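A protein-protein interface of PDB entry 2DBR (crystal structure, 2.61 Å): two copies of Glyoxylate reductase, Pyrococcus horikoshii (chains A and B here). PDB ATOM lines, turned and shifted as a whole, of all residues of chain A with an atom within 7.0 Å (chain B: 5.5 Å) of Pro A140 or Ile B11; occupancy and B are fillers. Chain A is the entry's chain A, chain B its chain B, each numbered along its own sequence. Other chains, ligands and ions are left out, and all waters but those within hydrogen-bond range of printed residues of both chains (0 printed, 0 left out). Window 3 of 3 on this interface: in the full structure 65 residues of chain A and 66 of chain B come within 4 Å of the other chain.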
ATOM      1  N   TRP A 138      24.893 -36.125 -11.172  1.00  0.00           N
ATOM      2  CA  TRP A 138      25.267 -34.798 -10.703  1.00  0.00           C
ATOM      3  C   TRP A 138      24.594 -33.716 -11.549  1.00  0.00           C
ATOM      4  O   TRP A 138      24.815 -33.642 -12.756  1.00  0.00           O
ATOM      5  CB  TRP A 138      26.792 -34.661 -10.794  1.00  0.00           C
ATOM      6  CG  TRP A 138      27.401 -33.423 -10.166  1.00  0.00           C
ATOM      7  CD1 TRP A 138      28.121 -33.363  -9.005  1.00  0.00           C
ATOM      8  CD2 TRP A 138      27.404 -32.093 -10.706  1.00  0.00           C
ATOM      9  NE1 TRP A 138      28.580 -32.086  -8.793  1.00  0.00           N
ATOM     10  CE2 TRP A 138      28.153 -31.285  -9.820  1.00  0.00           C
ATOM     11  CE3 TRP A 138      26.847 -31.506 -11.852  1.00  0.00           C
ATOM     12  CZ2 TRP A 138      28.362 -29.919 -10.046  1.00  0.00           C
ATOM     13  CZ3 TRP A 138      27.054 -30.148 -12.076  1.00  0.00           C
ATOM     14  CH2 TRP A 138      27.807 -29.369 -11.175  1.00  0.00           C
ATOM     15  N   HIS A 139      23.773 -32.878 -10.918  1.00  0.00           N
ATOM     16  CA  HIS A 139      23.095 -31.804 -11.643  1.00  0.00           C
ATOM     17  C   HIS A 139      23.514 -30.428 -11.120  1.00  0.00           C
ATOM     18  O   HIS A 139      23.705 -30.238  -9.921  1.00  0.00           O
ATOM     19  CB  HIS A 139      21.573 -31.950 -11.536  1.00  0.00           C
ATOM     20  CG  HIS A 139      20.817 -31.011 -12.428  1.00  0.00           C
ATOM     21  ND1 HIS A 139      20.660 -31.233 -13.780  1.00  0.00           N
ATOM     22  CD2 HIS A 139      20.224 -29.821 -12.172  1.00  0.00           C
ATOM     23  CE1 HIS A 139      20.004 -30.220 -14.318  1.00  0.00           C
ATOM     24  NE2 HIS A 139      19.729 -29.349 -13.365  1.00  0.00           N
ATOM     25  N   PRO A 140      23.654 -29.448 -12.023  1.00  0.00           N
ATOM     26  CA  PRO A 140      24.054 -28.084 -11.668  1.00  0.00           C
ATOM     27  C   PRO A 140      23.143 -27.369 -10.676  1.00  0.00           C
ATOM     28  O   PRO A 140      23.558 -26.401 -10.037  1.00  0.00           O
ATOM     29  CB  PRO A 140      24.073 -27.364 -13.016  1.00  0.00           C
ATOM     30  CG  PRO A 140      24.383 -28.458 -13.984  1.00  0.00           C
ATOM     31  CD  PRO A 140      23.527 -29.586 -13.484  1.00  0.00           C
ATOM     32  N   LYS A 141      21.910 -27.839 -10.533  1.00  0.00           N
ATOM     33  CA  LYS A 141      20.971 -27.167  -9.647  1.00  0.00           C
ATOM     34  C   LYS A 141      20.433 -27.989  -8.486  1.00  0.00           C
ATOM     35  O   LYS A 141      19.580 -27.510  -7.745  1.00  0.00           O
ATOM     36  CB  LYS A 141      19.799 -26.633 -10.469  1.00  0.00           C
ATOM     37  CG  LYS A 141      20.174 -26.331 -11.910  1.00  0.00           C
ATOM     38  CD  LYS A 141      19.060 -25.639 -12.665  1.00  0.00           C
ATOM     39  CE  LYS A 141      18.992 -24.158 -12.316  1.00  0.00           C
ATOM     40  NZ  LYS A 141      17.789 -23.508 -12.918  1.00  0.00           N
ATOM     41  N   TRP A 142      20.920 -29.211  -8.309  1.00  0.00           N
ATOM     42  CA  TRP A 142      20.427 -30.041  -7.214  1.00  0.00           C
ATOM     43  C   TRP A 142      20.989 -29.701  -5.845  1.00  0.00           C
ATOM     44  O   TRP A 142      22.116 -29.227  -5.711  1.00  0.00           O
ATOM     45  CB  TRP A 142      20.694 -31.514  -7.500  1.00  0.00           C
ATOM     46  CG  TRP A 142      19.785 -32.095  -8.534  1.00  0.00           C
ATOM     47  CD1 TRP A 142      19.075 -31.413  -9.483  1.00  0.00           C
ATOM     48  CD2 TRP A 142      19.536 -33.484  -8.770  1.00  0.00           C
ATOM     49  NE1 TRP A 142      18.406 -32.293 -10.298  1.00  0.00           N
ATOM     50  CE2 TRP A 142      18.671 -33.569  -9.881  1.00  0.00           C
ATOM     51  CE3 TRP A 142      19.962 -34.664  -8.150  1.00  0.00           C
ATOM     52  CZ2 TRP A 142      18.226 -34.787 -10.387  1.00  0.00           C
ATOM     53  CZ3 TRP A 142      19.518 -35.879  -8.653  1.00  0.00           C
ATOM     54  CH2 TRP A 142      18.658 -35.930  -9.761  1.00  0.00           C
ATOM     55  N   LEU A 144      20.902 -27.329  -3.840  1.00  0.00           N
ATOM     56  CA  LEU A 144      21.477 -26.024  -3.529  1.00  0.00           C
ATOM     57  C   LEU A 144      21.246 -25.693  -2.050  1.00  0.00           C
ATOM     58  O   LEU A 144      20.145 -25.874  -1.518  1.00  0.00           O
ATOM     59  CB  LEU A 144      20.850 -24.936  -4.400  1.00  0.00           C
ATOM     60  CG  LEU A 144      21.672 -24.543  -5.626  1.00  0.00           C
ATOM     61  CD1 LEU A 144      22.077 -25.794  -6.371  1.00  0.00           C
ATOM     62  CD2 LEU A 144      20.866 -23.611  -6.526  1.00  0.00           C
ATOM     63  N   ILE B   7      25.975 -26.407 -24.409  1.00  0.00           N
ATOM     64  CA  ILE B   7      26.075 -26.571 -22.965  1.00  0.00           C
ATOM     65  C   ILE B   7      25.385 -27.867 -22.551  1.00  0.00           C
ATOM     66  O   ILE B   7      24.161 -27.970 -22.588  1.00  0.00           O
ATOM     67  CB  ILE B   7      25.440 -25.371 -22.249  1.00  0.00           C
ATOM     68  CG1 ILE B   7      26.149 -24.093 -22.701  1.00  0.00           C
ATOM     69  CG2 ILE B   7      25.538 -25.544 -20.743  1.00  0.00           C
ATOM     70  CD1 ILE B   7      25.549 -22.811 -22.165  1.00  0.00           C
ATOM     71  N   ARG B   9      24.448 -29.218 -19.890  1.00  0.00           N
ATOM     72  CA  ARG B   9      23.384 -29.242 -18.890  1.00  0.00           C
ATOM     73  C   ARG B   9      22.903 -27.855 -18.485  1.00  0.00           C
ATOM     74  O   ARG B   9      23.600 -26.857 -18.664  1.00  0.00           O
ATOM     75  CB  ARG B   9      23.844 -29.996 -17.643  1.00  0.00           C
ATOM     76  CG  ARG B   9      22.712 -30.466 -16.748  1.00  0.00           C
ATOM     77  CD  ARG B   9      22.044 -31.698 -17.334  1.00  0.00           C
ATOM     78  NE  ARG B   9      23.001 -32.789 -17.504  1.00  0.00           N
ATOM     79  CZ  ARG B   9      23.612 -33.406 -16.500  1.00  0.00           C
ATOM     80  NH1 ARG B   9      23.366 -33.044 -15.251  1.00  0.00           N
ATOM     81  NH2 ARG B   9      24.480 -34.377 -16.742  1.00  0.00           N
ATOM     82  N   GLU B  10      21.696 -27.814 -17.932  1.00  0.00           N
ATOM     83  CA  GLU B  10      21.073 -26.575 -17.482  1.00  0.00           C
ATOM     84  C   GLU B  10      21.816 -25.978 -16.286  1.00  0.00           C
ATOM     85  O   GLU B  10      21.711 -26.494 -15.174  1.00  0.00           O
ATOM     86  CB  GLU B  10      19.615 -26.858 -17.097  1.00  0.00           C
ATOM     87  CG  GLU B  10      18.931 -25.748 -16.318  1.00  0.00           C
ATOM     88  CD  GLU B  10      17.585 -26.180 -15.760  1.00  0.00           C
ATOM     89  OE1 GLU B  10      17.532 -27.222 -15.069  1.00  0.00           O
ATOM     90  OE2 GLU B  10      16.581 -25.477 -16.005  1.00  0.00           O
ATOM     91  N   ILE B  11      22.568 -24.903 -16.509  1.00  0.00           N
ATOM     92  CA  ILE B  11      23.295 -24.274 -15.411  1.00  0.00           C
ATOM     93  C   ILE B  11      22.783 -22.852 -15.181  1.00  0.00           C
ATOM     94  O   ILE B  11      22.131 -22.276 -16.050  1.00  0.00           O
ATOM     95  CB  ILE B  11      24.846 -24.247 -15.666  1.00  0.00           C
ATOM     96  CG1 ILE B  11      25.263 -23.002 -16.465  1.00  0.00           C
ATOM     97  CG2 ILE B  11      25.277 -25.523 -16.372  1.00  0.00           C
ATOM     98  CD1 ILE B  11      24.971 -23.044 -17.944  1.00  0.00           C
ATOM     99  N   PRO B  12      23.066 -22.272 -14.001  1.00  0.00           N
ATOM    100  CA  PRO B  12      22.637 -20.916 -13.650  1.00  0.00           C
ATOM    101  C   PRO B  12      22.410 -19.964 -14.826  1.00  0.00           C
ATOM    102  O   PRO B  12      23.262 -19.811 -15.704  1.00  0.00           O
ATOM    103  CB  PRO B  12      23.745 -20.456 -12.718  1.00  0.00           C
ATOM    104  CG  PRO B  12      23.982 -21.698 -11.918  1.00  0.00           C
ATOM    105  CD  PRO B  12      23.956 -22.813 -12.957  1.00  0.00           C
ATOM    106  N   GLU B  13      21.243 -19.325 -14.818  1.00  0.00           N
ATOM    107  CA  GLU B  13      20.839 -18.385 -15.860  1.00  0.00           C
ATOM    108  C   GLU B  13      21.883 -17.301 -16.110  1.00  0.00           C
ATOM    109  O   GLU B  13      22.091 -16.887 -17.246  1.00  0.00           O
ATOM    110  CB  GLU B  13      19.509 -17.726 -15.473  1.00  0.00           C
ATOM    111  CG  GLU B  13      18.749 -17.109 -16.639  1.00  0.00           C
ATOM    112  CD  GLU B  13      18.082 -18.154 -17.526  1.00  0.00           C
ATOM    113  OE1 GLU B  13      17.165 -18.852 -17.040  1.00  0.00           O
ATOM    114  OE2 GLU B  13      18.478 -18.279 -18.705  1.00  0.00           O
ATOM    115  N   GLY B  15      24.920 -17.371 -16.358  1.00  0.00           N
ATOM    116  CA  GLY B  15      25.904 -17.769 -17.348  1.00  0.00           C
ATOM    117  C   GLY B  15      25.339 -17.789 -18.755  1.00  0.00           C
ATOM    118  O   GLY B  15      25.897 -17.173 -19.665  1.00  0.00           O
ATOM    119  N   ILE B  16      24.230 -18.502 -18.930  1.00  0.00           N
ATOM    120  CA  ILE B  16      23.576 -18.608 -20.228  1.00  0.00           C
ATOM    121  C   ILE B  16      23.422 -17.226 -20.872  1.00  0.00           C
ATOM    122  O   ILE B  16      23.486 -17.092 -22.092  1.00  0.00           O
ATOM    123  CB  ILE B  16      22.170 -19.243 -20.093  1.00  0.00           C
ATOM    124  CG1 ILE B  16      22.248 -20.556 -19.311  1.00  0.00           C
ATOM    125  CG2 ILE B  16      21.583 -19.500 -21.472  1.00  0.00           C
ATOM    126  CD1 ILE B  16      22.918 -21.679 -20.057  1.00  0.00           C
ATOM    127  N   VAL B  27      21.198 -25.393 -25.214  1.00  0.00           N
ATOM    128  CA  VAL B  27      21.320 -26.038 -23.917  1.00  0.00           C
ATOM    129  C   VAL B  27      20.608 -27.377 -23.811  1.00  0.00           C
ATOM    130  O   VAL B  27      19.381 -27.432 -23.852  1.00  0.00           O
ATOM    131  CB  VAL B  27      20.775 -25.116 -22.797  1.00  0.00           C
ATOM    132  CG1 VAL B  27      20.873 -25.812 -21.450  1.00  0.00           C
ATOM    133  CG2 VAL B  27      21.546 -23.806 -22.774  1.00  0.00           C
ATOM    134  N   VAL B  50      30.438 -26.570 -23.076  1.00  0.00           N
ATOM    135  CA  VAL B  50      30.339 -26.477 -21.627  1.00  0.00           C
ATOM    136  C   VAL B  50      29.872 -27.847 -21.152  1.00  0.00           C
ATOM    137  O   VAL B  50      28.751 -28.272 -21.438  1.00  0.00           O
ATOM    138  CB  VAL B  50      29.337 -25.389 -21.183  1.00  0.00           C
ATOM    139  CG1 VAL B  50      29.047 -25.536 -19.705  1.00  0.00           C
ATOM    140  CG2 VAL B  50      29.912 -23.998 -21.461  1.00  0.00           C
ATOM    141  N   MET B  52      29.748 -31.072 -17.986  1.00  0.00           N
ATOM    142  CA  MET B  52      29.591 -31.362 -16.566  1.00  0.00           C
ATOM    143  C   MET B  52      30.568 -32.491 -16.254  1.00  0.00           C
ATOM    144  O   MET B  52      31.108 -33.118 -17.165  1.00  0.00           O
ATOM    145  CB  MET B  52      28.167 -31.843 -16.247  1.00  0.00           C
ATOM    146  CG  MET B  52      27.049 -30.908 -16.675  1.00  0.00           C
ATOM    147  SD  MET B  52      27.214 -29.266 -15.982  1.00  0.00           S
ATOM    148  CE  MET B  52      27.827 -28.316 -17.412  1.00  0.00           C
ATOM    149  N   TYR B  74      32.326 -27.266 -16.231  1.00  0.00           N
ATOM    150  CA  TYR B  74      31.582 -26.639 -15.141  1.00  0.00           C
ATOM    151  C   TYR B  74      31.917 -27.476 -13.916  1.00  0.00           C
ATOM    152  O   TYR B  74      31.104 -28.258 -13.416  1.00  0.00           O
ATOM    153  CB  TYR B  74      30.075 -26.665 -15.429  1.00  0.00           C
ATOM    154  CG  TYR B  74      29.216 -25.906 -14.432  1.00  0.00           C
ATOM    155  CD1 TYR B  74      28.356 -26.587 -13.563  1.00  0.00           C
ATOM    156  CD2 TYR B  74      29.251 -24.511 -14.363  1.00  0.00           C
ATOM    157  CE1 TYR B  74      27.550 -25.894 -12.653  1.00  0.00           C
ATOM    158  CE2 TYR B  74      28.450 -23.808 -13.457  1.00  0.00           C
ATOM    159  CZ  TYR B  74      27.604 -24.508 -12.607  1.00  0.00           C
ATOM    160  OH  TYR B  74      26.824 -23.825 -11.703  1.00  0.00           O
ATOM    161  N   ARG B 297      27.524 -22.407  -7.452  1.00  0.00           N
ATOM    162  CA  ARG B 297      27.000 -22.732  -8.769  1.00  0.00           C
ATOM    163  C   ARG B 297      26.777 -21.440  -9.560  1.00  0.00           C
ATOM    164  O   ARG B 297      26.739 -21.439 -10.796  1.00  0.00           O
ATOM    165  CB  ARG B 297      25.683 -23.490  -8.629  1.00  0.00           C
ATOM    166  CG  ARG B 297      25.770 -24.774  -7.809  1.00  0.00           C
ATOM    167  CD  ARG B 297      26.434 -25.929  -8.570  1.00  0.00           C
ATOM    168  NE  ARG B 297      25.771 -27.189  -8.236  1.00  0.00           N
ATOM    169  CZ  ARG B 297      26.354 -28.217  -7.630  1.00  0.00           C
ATOM    170  NH1 ARG B 297      27.631 -28.155  -7.285  1.00  0.00           N
ATOM    171  NH2 ARG B 297      25.650 -29.307  -7.350  1.00  0.00           N
ATOM    172  N   ALA B 301      29.192 -20.488 -12.788  1.00  0.00           N
ATOM    173  CA  ALA B 301      28.514 -20.155 -14.033  1.00  0.00           C
ATOM    174  C   ALA B 301      29.129 -18.929 -14.708  1.00  0.00           C
ATOM    175  O   ALA B 301      29.359 -18.933 -15.918  1.00  0.00           O
ATOM    176  CB  ALA B 301      27.039 -19.926 -13.771  1.00  0.00           C
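The side-chain hydroxyl of Tyr B74 lies within hydrogen-bond range of the backbone carbonyl oxygen of Arg B297.
Among the printed residues, merely in contact across the chains: Pro A140 with Glu B10 (3.3 Å), Trp A138 with Arg B297 (3.4 Å), Pro A140 with Arg B9 (3.5 Å), His A139 with Glu B10 (3.5 Å), Pro A140 with Met B52 (3.6 Å), His A139 with Arg B9 (3.6 Å), Trp A138 with Tyr B74 (3.7 Å), Pro A140 with Tyr B74 (3.8 Å), Pro A140 with Ile B11 (3.9 Å) and Trp A142 with Arg B297 (3.9 Å).
Printed residues of chain B within 4 Å of Trp A138: Arg B9, Tyr B74 and Arg B297.
Of chain B, only Arg B9, Glu B10, Ile B11, Met B52, Tyr B74 and Arg B297 come within 4 Å of Pro A140.
Ile B7 touches none of the printed residues of chain A.
Of the printed residues of chain A, Glu B10 touches His A139, Pro A140 and Lys A141.
Ile B11 touches one residue of chain A.
Printed residues of chain A within 4 Å of Met B52: Pro A140.
Printed residues of chain A within 4 Å of Tyr B74: Trp A138 and Pro A140.
No position is printed for both chains.
Of the 14 pairs that touch across the chains among the printed residues, none has its exchanged pair printed and touching as well.
Of the 6 printed residues of chain A, 5 touch a printed residue of chain B.
Hydrophobic or aromatic side chains of chain A that line the printed part of chain B: Trp A138, His A139 and Pro A140.
Printed residues of chain B that touch a printed residue of chain A: Arg B9, Glu B10, Ile B11, Met B52, Tyr B74 and Arg B297.
Hydrophobic or aromatic side chains of chain B that line the printed part of chain A: Ile B11, Met B52 and Tyr B74.
Among the printed residues, 14 pairs touch across the chains.
The backbone carbonyl oxygen (O) of Trp A138 lies within hydrogen-bond range of the guanidinium group (NH1) of Arg B9.
O of His A139 sits at hydrogen-bond distance from NH2 of Arg B297 (3.4 Å).
The guanidinium group (NE) of Arg B297 is in hydrogen-bond range of the backbone carbonyl oxygen (O) of Pro A140 (3.0 Å).
The side-chain amino group of Lys A141 lies within salt-bridge range of the side-chain carboxylate of Glu B10 (3.9 Å).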
